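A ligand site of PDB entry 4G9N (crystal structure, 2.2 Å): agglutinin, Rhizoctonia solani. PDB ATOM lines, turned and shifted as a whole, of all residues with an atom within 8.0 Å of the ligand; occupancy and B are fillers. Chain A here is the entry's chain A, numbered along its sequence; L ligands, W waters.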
ATOM      1  N   VAL A  20      20.284  18.108  32.554  1.00  0.00           N
ATOM      2  CA  VAL A  20      19.597  18.927  31.557  1.00  0.00           C
ATOM      3  C   VAL A  20      20.291  18.957  30.195  1.00  0.00           C
ATOM      4  O   VAL A  20      21.474  18.648  30.084  1.00  0.00           O
ATOM      5  CB  VAL A  20      19.399  20.367  32.068  1.00  0.00           C
ATOM      6  CG1 VAL A  20      18.639  20.347  33.378  1.00  0.00           C
ATOM      7  CG2 VAL A  20      20.737  21.061  32.244  1.00  0.00           C
ATOM      8  N   LEU A  21      19.527  19.345  29.173  1.00  0.00           N
ATOM      9  CA  LEU A  21      20.050  19.502  27.814  1.00  0.00           C
ATOM     10  C   LEU A  21      21.088  20.629  27.757  1.00  0.00           C
ATOM     11  O   LEU A  21      20.796  21.777  28.096  1.00  0.00           O
ATOM     12  CB  LEU A  21      18.907  19.784  26.822  1.00  0.00           C
ATOM     13  CG  LEU A  21      19.211  19.520  25.346  1.00  0.00           C
ATOM     14  CD1 LEU A  21      19.312  18.026  25.104  1.00  0.00           C
ATOM     15  CD2 LEU A  21      18.152  20.129  24.451  1.00  0.00           C
ATOM     16  N   ASP A  22      22.287  20.290  27.290  1.00  0.00           N
ATOM     17  CA  ASP A  22      23.451  21.144  27.445  1.00  0.00           C
ATOM     18  C   ASP A  22      24.212  21.183  26.138  1.00  0.00           C
ATOM     19  O   ASP A  22      24.527  20.134  25.577  1.00  0.00           O
ATOM     20  CB  ASP A  22      24.365  20.585  28.551  1.00  0.00           C
ATOM     21  CG  ASP A  22      25.533  21.509  28.891  1.00  0.00           C
ATOM     22  OD1 ASP A  22      25.525  22.115  29.980  1.00  0.00           O
ATOM     23  OD2 ASP A  22      26.478  21.612  28.073  1.00  0.00           O
ATOM     24  N   LEU A  23      24.489  22.386  25.647  1.00  0.00           N
ATOM     25  CA  LEU A  23      25.336  22.524  24.459  1.00  0.00           C
ATOM     26  C   LEU A  23      26.749  22.800  24.932  1.00  0.00           C
ATOM     27  O   LEU A  23      26.982  23.751  25.682  1.00  0.00           O
ATOM     28  CB  LEU A  23      24.844  23.657  23.553  1.00  0.00           C
ATOM     29  CG  LEU A  23      25.694  23.847  22.302  1.00  0.00           C
ATOM     30  CD1 LEU A  23      25.362  22.817  21.254  1.00  0.00           C
ATOM     31  CD2 LEU A  23      25.539  25.227  21.733  1.00  0.00           C
ATOM     32  N   TRP A  24      27.685  21.967  24.484  1.00  0.00           N
ATOM     33  CA  TRP A  24      29.056  21.990  24.959  1.00  0.00           C
ATOM     34  C   TRP A  24      29.662  23.405  24.893  1.00  0.00           C
ATOM     35  O   TRP A  24      29.860  23.948  23.817  1.00  0.00           O
ATOM     36  CB  TRP A  24      29.893  21.010  24.140  1.00  0.00           C
ATOM     37  CG  TRP A  24      31.313  20.850  24.607  1.00  0.00           C
ATOM     38  CD1 TRP A  24      31.792  19.917  25.478  1.00  0.00           C
ATOM     39  CD2 TRP A  24      32.437  21.637  24.213  1.00  0.00           C
ATOM     40  NE1 TRP A  24      33.136  20.082  25.654  1.00  0.00           N
ATOM     41  CE2 TRP A  24      33.558  21.136  24.884  1.00  0.00           C
ATOM     42  CE3 TRP A  24      32.596  22.733  23.351  1.00  0.00           C
ATOM     43  CZ2 TRP A  24      34.833  21.683  24.736  1.00  0.00           C
ATOM     44  CZ3 TRP A  24      33.859  23.273  23.193  1.00  0.00           C
ATOM     45  CH2 TRP A  24      34.952  22.749  23.884  1.00  0.00           C
ATOM     46  N   ARG A  25      29.907  23.977  26.077  1.00  0.00           N
ATOM     47  CA  ARG A  25      30.418  25.349  26.220  1.00  0.00           C
ATOM     48  C   ARG A  25      29.652  26.424  25.461  1.00  0.00           C
ATOM     49  O   ARG A  25      30.182  27.516  25.216  1.00  0.00           O
ATOM     50  CB  ARG A  25      31.880  25.427  25.824  1.00  0.00           C
ATOM     51  CG  ARG A  25      32.794  24.642  26.706  1.00  0.00           C
ATOM     52  CD  ARG A  25      34.195  25.182  26.521  1.00  0.00           C
ATOM     53  NE  ARG A  25      35.191  24.353  27.171  1.00  0.00           N
ATOM     54  CZ  ARG A  25      36.490  24.519  26.994  1.00  0.00           C
ATOM     55  NH1 ARG A  25      36.939  25.495  26.197  1.00  0.00           N
ATOM     56  NH2 ARG A  25      37.352  23.718  27.625  1.00  0.00           N
ATOM     57  N   GLY A  26      28.413  26.137  25.087  1.00  0.00           N
ATOM     58  CA  GLY A  26      27.618  27.088  24.341  1.00  0.00           C
ATOM     59  C   GLY A  26      28.314  27.520  23.060  1.00  0.00           C
ATOM     60  O   GLY A  26      28.089  28.633  22.587  1.00  0.00           O
ATOM     61  N   GLU A  27      29.134  26.628  22.504  1.00  0.00           N
ATOM     62  CA  GLU A  27      29.918  26.886  21.283  1.00  0.00           C
ATOM     63  C   GLU A  27      29.059  26.864  20.007  1.00  0.00           C
ATOM     64  O   GLU A  27      28.278  25.940  19.782  1.00  0.00           O
ATOM     65  CB  GLU A  27      31.046  25.859  21.166  1.00  0.00           C
ATOM     66  CG  GLU A  27      32.441  26.465  21.013  1.00  0.00           C
ATOM     67  CD  GLU A  27      32.488  27.593  19.986  1.00  0.00           C
ATOM     68  OE1 GLU A  27      32.381  27.308  18.764  1.00  0.00           O
ATOM     69  OE2 GLU A  27      32.640  28.765  20.407  1.00  0.00           O
ATOM     70  N   THR A  32      28.820  21.051  17.235  1.00  0.00           N
ATOM     71  CA  THR A  32      29.123  21.054  18.660  1.00  0.00           C
ATOM     72  C   THR A  32      28.202  20.093  19.387  1.00  0.00           C
ATOM     73  O   THR A  32      27.012  20.007  19.072  1.00  0.00           O
ATOM     74  CB  THR A  32      29.019  22.463  19.277  1.00  0.00           C
ATOM     75  OG1 THR A  32      29.996  23.320  18.678  1.00  0.00           O
ATOM     76  CG2 THR A  32      29.291  22.413  20.778  1.00  0.00           C
ATOM     77  N   ALA A  33      28.773  19.365  20.343  1.00  0.00           N
ATOM     78  CA  ALA A  33      28.045  18.346  21.087  1.00  0.00           C
ATOM     79  C   ALA A  33      26.861  18.881  21.892  1.00  0.00           C
ATOM     80  O   ALA A  33      26.943  19.911  22.563  1.00  0.00           O
ATOM     81  CB  ALA A  33      28.994  17.604  22.003  1.00  0.00           C
ATOM     82  N   GLN A  35      24.364  17.379  24.914  1.00  0.00           N
ATOM     83  CA  GLN A  35      24.650  16.386  25.932  1.00  0.00           C
ATOM     84  C   GLN A  35      23.815  16.599  27.200  1.00  0.00           C
ATOM     85  O   GLN A  35      23.145  17.617  27.350  1.00  0.00           O
ATOM     86  CB  GLN A  35      26.147  16.487  26.282  1.00  0.00           C
ATOM     87  CG  GLN A  35      26.500  17.873  26.847  1.00  0.00           C
ATOM     88  CD  GLN A  35      27.997  18.107  26.953  1.00  0.00           C
ATOM     89  OE1 GLN A  35      28.791  17.288  26.506  1.00  0.00           O
ATOM     90  NE2 GLN A  35      28.391  19.234  27.540  1.00  0.00           N
ATOM     91  N   GLY A  36      23.874  15.630  28.108  1.00  0.00           N
ATOM     92  CA  GLY A  36      23.320  15.815  29.438  1.00  0.00           C
ATOM     93  C   GLY A  36      24.367  16.411  30.350  1.00  0.00           C
ATOM     94  O   GLY A  36      25.557  16.117  30.210  1.00  0.00           O
ATOM     95  N   TYR A  37      23.948  17.257  31.287  1.00  0.00           N
ATOM     96  CA  TYR A  37      24.883  17.920  32.185  1.00  0.00           C
ATOM     97  C   TYR A  37      24.116  18.422  33.413  1.00  0.00           C
ATOM     98  O   TYR A  37      22.936  18.756  33.313  1.00  0.00           O
ATOM     99  CB  TYR A  37      25.556  19.098  31.476  1.00  0.00           C
ATOM    100  CG  TYR A  37      26.937  19.446  32.006  1.00  0.00           C
ATOM    101  CD1 TYR A  37      27.091  20.291  33.095  1.00  0.00           C
ATOM    102  CD2 TYR A  37      28.075  18.940  31.395  1.00  0.00           C
ATOM    103  CE1 TYR A  37      28.345  20.609  33.585  1.00  0.00           C
ATOM    104  CE2 TYR A  37      29.348  19.259  31.873  1.00  0.00           C
ATOM    105  CZ  TYR A  37      29.473  20.094  32.964  1.00  0.00           C
ATOM    106  OH  TYR A  37      30.736  20.424  33.444  1.00  0.00           O
ATOM    107  N   LYS A  38      24.778  18.440  34.570  1.00  0.00           N
ATOM    108  CA  LYS A  38      24.169  18.992  35.776  1.00  0.00           C
ATOM    109  C   LYS A  38      23.718  20.441  35.564  1.00  0.00           C
ATOM    110  O   LYS A  38      24.420  21.237  34.949  1.00  0.00           O
ATOM    111  CB  LYS A  38      25.109  18.851  36.983  1.00  0.00           C
ATOM    112  CG  LYS A  38      25.117  17.449  37.586  1.00  0.00           C
ATOM    113  CD  LYS A  38      26.431  17.094  38.258  1.00  0.00           C
ATOM    114  CE  LYS A  38      26.339  15.789  39.025  1.00  0.00           C
ATOM    115  NZ  LYS A  38      25.178  14.964  38.578  1.00  0.00           N
ATOM    116  N   SER A  39      22.534  20.754  36.065  1.00  0.00           N
ATOM    117  CA  SER A  39      21.911  22.055  35.859  1.00  0.00           C
ATOM    118  C   SER A  39      22.637  23.167  36.595  1.00  0.00           C
ATOM    119  O   SER A  39      22.673  23.179  37.830  1.00  0.00           O
ATOM    120  CB  SER A  39      20.458  21.985  36.328  1.00  0.00           C
ATOM    121  OG  SER A  39      19.808  23.230  36.156  1.00  0.00           O
ATOM    122  N   HIS A  40      23.203  24.121  35.851  1.00  0.00           N
ATOM    123  CA  HIS A  40      23.836  25.272  36.493  1.00  0.00           C
ATOM    124  C   HIS A  40      23.198  26.615  36.163  1.00  0.00           C
ATOM    125  O   HIS A  40      23.665  27.652  36.612  1.00  0.00           O
ATOM    126  CB  HIS A  40      25.343  25.308  36.216  1.00  0.00           C
ATOM    127  CG  HIS A  40      25.692  25.211  34.764  1.00  0.00           C
ATOM    128  ND1 HIS A  40      25.204  26.095  33.824  1.00  0.00           N
ATOM    129  CD2 HIS A  40      26.508  24.359  34.093  1.00  0.00           C
ATOM    130  CE1 HIS A  40      25.695  25.778  32.632  1.00  0.00           C
ATOM    131  NE2 HIS A  40      26.492  24.737  32.769  1.00  0.00           N
ATOM    132  N   GLY A  41      22.127  26.589  35.363  1.00  0.00           N
ATOM    133  CA  GLY A  41      21.381  27.797  35.065  1.00  0.00           C
ATOM    134  C   GLY A  41      21.953  28.698  33.973  1.00  0.00           C
ATOM    135  O   GLY A  41      21.353  29.725  33.645  1.00  0.00           O
ATOM    136  N   GLY A  42      23.099  28.325  33.415  1.00  0.00           N
ATOM    137  CA  GLY A  42      23.725  29.117  32.359  1.00  0.00           C
ATOM    138  C   GLY A  42      22.961  29.060  31.034  1.00  0.00           C
ATOM    139  O   GLY A  42      22.189  28.137  30.797  1.00  0.00           O
ATOM    140  N   ASP A  43      23.181  30.051  30.186  1.00  0.00           N
ATOM    141  CA  ASP A  43      22.454  30.146  28.914  1.00  0.00           C
ATOM    142  C   ASP A  43      22.705  28.987  27.934  1.00  0.00           C
ATOM    143  O   ASP A  43      21.878  28.710  27.080  1.00  0.00           O
ATOM    144  CB  ASP A  43      22.730  31.491  28.244  1.00  0.00           C
ATOM    145  CG  ASP A  43      22.062  32.646  28.959  1.00  0.00           C
ATOM    146  OD1 ASP A  43      21.074  32.409  29.678  1.00  0.00           O
ATOM    147  OD2 ASP A  43      22.533  33.786  28.802  1.00  0.00           O
ATOM    148  N   ASN A  44      23.818  28.292  28.081  1.00  0.00           N
ATOM    149  CA  ASN A  44      24.056  27.130  27.234  1.00  0.00           C
ATOM    150  C   ASN A  44      23.162  25.941  27.632  1.00  0.00           C
ATOM    151  O   ASN A  44      23.129  24.910  26.955  1.00  0.00           O
ATOM    152  CB  ASN A  44      25.539  26.739  27.265  1.00  0.00           C
ATOM    153  CG  ASN A  44      25.968  26.165  28.594  1.00  0.00           C
ATOM    154  OD1 ASN A  44      25.612  26.685  29.650  1.00  0.00           O
ATOM    155  ND2 ASN A  44      26.731  25.076  28.543  1.00  0.00           N
ATOM    156  N   GLN A  45      22.428  26.096  28.744  1.00  0.00           N
ATOM    157  CA  GLN A  45      21.446  25.100  29.155  1.00  0.00           C
ATOM    158  C   GLN A  45      20.019  25.631  29.009  1.00  0.00           C
ATOM    159  O   GLN A  45      19.102  25.149  29.665  1.00  0.00           O
ATOM    160  CB  GLN A  45      21.706  24.625  30.584  1.00  0.00           C
ATOM    161  CG  GLN A  45      22.982  23.831  30.744  1.00  0.00           C
ATOM    162  CD  GLN A  45      23.244  23.416  32.183  1.00  0.00           C
ATOM    163  OE1 GLN A  45      22.702  24.002  33.121  1.00  0.00           O
ATOM    164  NE2 GLN A  45      24.077  22.398  32.361  1.00  0.00           N
ATOM    165  N   LYS A  64      22.549  30.537  24.347  1.00  0.00           N
ATOM    166  CA  LYS A  64      23.956  30.932  24.298  1.00  0.00           C
ATOM    167  C   LYS A  64      24.530  30.998  22.867  1.00  0.00           C
ATOM    168  O   LYS A  64      24.975  32.055  22.432  1.00  0.00           O
ATOM    169  CB  LYS A  64      24.807  29.980  25.160  1.00  0.00           C
ATOM    170  CG  LYS A  64      26.267  30.415  25.286  1.00  0.00           C
ATOM    171  CD  LYS A  64      26.339  31.885  25.697  1.00  0.00           C
ATOM    172  CE  LYS A  64      27.754  32.427  25.622  1.00  0.00           C
ATOM    173  NZ  LYS A  64      27.751  33.902  25.839  1.00  0.00           N
ATOM    174  N   ASN A 120      27.928  13.831  33.644  1.00  0.00           N
ATOM    175  CA  ASN A 120      28.173  15.009  32.826  1.00  0.00           C
ATOM    176  C   ASN A 120      28.776  14.632  31.487  1.00  0.00           C
ATOM    177  O   ASN A 120      29.661  13.794  31.433  1.00  0.00           O
ATOM    178  CB  ASN A 120      29.124  15.982  33.509  1.00  0.00           C
ATOM    179  CG  ASN A 120      28.426  16.817  34.561  1.00  0.00           C
ATOM    180  OD1 ASN A 120      27.204  16.978  34.529  1.00  0.00           O
ATOM    181  ND2 ASN A 120      29.203  17.357  35.488  1.00  0.00           N
ATOM    182  N   GLU A 121      28.273  15.282  30.436  1.00  0.00           N
ATOM    183  CA  GLU A 121      28.752  15.117  29.068  1.00  0.00           C
ATOM    184  C   GLU A 121      28.331  13.785  28.439  1.00  0.00           C
ATOM    185  O   GLU A 121      28.907  13.350  27.442  1.00  0.00           O
ATOM    186  CB  GLU A 121      30.273  15.335  28.965  1.00  0.00           C
ATOM    187  CG  GLU A 121      30.718  16.730  29.458  1.00  0.00           C
ATOM    188  CD  GLU A 121      32.210  16.981  29.292  1.00  0.00           C
ATOM    189  OE1 GLU A 121      32.967  16.016  29.110  1.00  0.00           O
ATOM    190  OE2 GLU A 121      32.619  18.145  29.361  1.00  0.00           O
ATOM    191  N   THR A 122      27.312  13.157  29.011  1.00  0.00           N
ATOM    192  CA  THR A 122      26.657  12.027  28.366  1.00  0.00           C
ATOM    193  C   THR A 122      25.975  12.566  27.104  1.00  0.00           C
ATOM    194  O   THR A 122      25.194  13.520  27.174  1.00  0.00           O
ATOM    195  CB  THR A 122      25.600  11.364  29.274  1.00  0.00           C
ATOM    196  OG1 THR A 122      26.223  10.849  30.466  1.00  0.00           O
ATOM    197  CG2 THR A 122      24.903  10.222  28.529  1.00  0.00           C
HETATM  198  C1  LIG L   1      31.184  24.066  30.698  1.00  0.00           C
HETATM  199  C2  LIG L   1      29.701  24.369  30.836  1.00  0.00           C
HETATM  200  C3  LIG L   1      28.866  23.084  30.830  1.00  0.00           C
HETATM  201  C4  LIG L   1      29.301  22.136  29.710  1.00  0.00           C
HETATM  202  C5  LIG L   1      30.818  21.988  29.676  1.00  0.00           C
HETATM  203  C6  LIG L   1      31.286  21.174  28.483  1.00  0.00           C
HETATM  204  C7  LIG L   1      29.087  26.309  32.172  1.00  0.00           C
HETATM  205  C8  LIG L   1      28.995  26.888  33.553  1.00  0.00           C
HETATM  206  N1  LIG L   1      29.503  25.052  32.095  1.00  0.00           N
HETATM  207  O1  LIG L   1      31.866  25.282  30.536  1.00  0.00           O
HETATM  208  O2  LIG L   1      27.494  23.420  30.807  1.00  0.00           O
HETATM  209  O3  LIG L   1      28.820  22.578  28.446  1.00  0.00           O
HETATM  210  O4  LIG L   1      31.439  23.245  29.581  1.00  0.00           O
HETATM  211  O5  LIG L   1      30.883  19.831  28.627  1.00  0.00           O
HETATM  212  O6  LIG L   1      28.792  26.976  31.170  1.00  0.00           O
HETATM  213  O   HOH W   1      30.870  23.777  34.410  1.00  0.00           O
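OD1 of Asp 22 is in hydrogen-bond range of O2 of the ligand, 2.5 Å away. O5 of the ligand sits at hydrogen-bond distance from OE2 of Glu 121, at 2.5 Å. An oxygen (O2) of the ligand lies within hydrogen-bond range of a ring nitrogen (NE2) of His 40. NE2 of Gln 35 lies within hydrogen-bond range of O5 of the ligand, at 2.8 Å. O2 of the ligand lies within hydrogen-bond range of ND2 of Asn 44 (2.9 Å). The backbone NH (N) of Arg 25 sits at hydrogen-bond distance from an oxygen (O3) of the ligand, at 3.0 Å.
The backbone NH (N) of Asp 22 lies within hydrogen-bond range of the backbone carbonyl oxygen (O) of Gln 35 (2.8 Å). The side-chain carboxylate (OD1) of Asp 22 sits at hydrogen-bond distance from the side-chain amide nitrogen (NE2) of Gln 45 (2.8 Å). The backbone NH (N) of Glu 121 sits at hydrogen-bond distance from the backbone carbonyl oxygen (O) of Gly 36 (2.9 Å). The side-chain amide oxygen (OE1) of Gln 45 lies within hydrogen-bond range of the backbone NH (N) of His 40, at 2.8 Å. A ring nitrogen (ND1) of His 40 sits at hydrogen-bond distance from the backbone NH (N) of Gly 42 (3.1 Å). N of Trp 24 sits at hydrogen-bond distance from O of Ala 33, at 2.9 Å. The backbone carbonyl oxygen (O) of Tyr 37 sits at hydrogen-bond distance from the backbone NH (N) of Val 20, 2.8 Å away. The side-chain amide nitrogen (NE2) of Gln 45 sits at hydrogen-bond distance from the backbone carbonyl oxygen (O) of Lys 38 (2.9 Å).
Water W1 bridges a nitrogen (N1) of the ligand (3.0 Å) and the side-chain hydroxyl of Tyr 37 (3.5 Å).
O of Leu 23 touches O3 of the ligand, 3.5 Å away. Trp 24 touches the ligand (CD1 to O5, 3.3 Å). CE2 of Tyr 37 touches C4 of the ligand (3.6 Å). NE2 of Gln 45 touches O2 of the ligand, 3.9 Å away. Hydrophobic or aromatic side chains within 4 Å of the ligand: Trp 24, Tyr 37 and His 40. Ten residues have an atom within 4 Å of the ligand: Asp 22, Leu 23, Trp 24, Arg 25, Gln 35, Tyr 37, His 40, Asn 44, Gln 45 and Glu 121. The nearest printed residue that does not touch the ligand is Gly 26 (4.9 Å).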
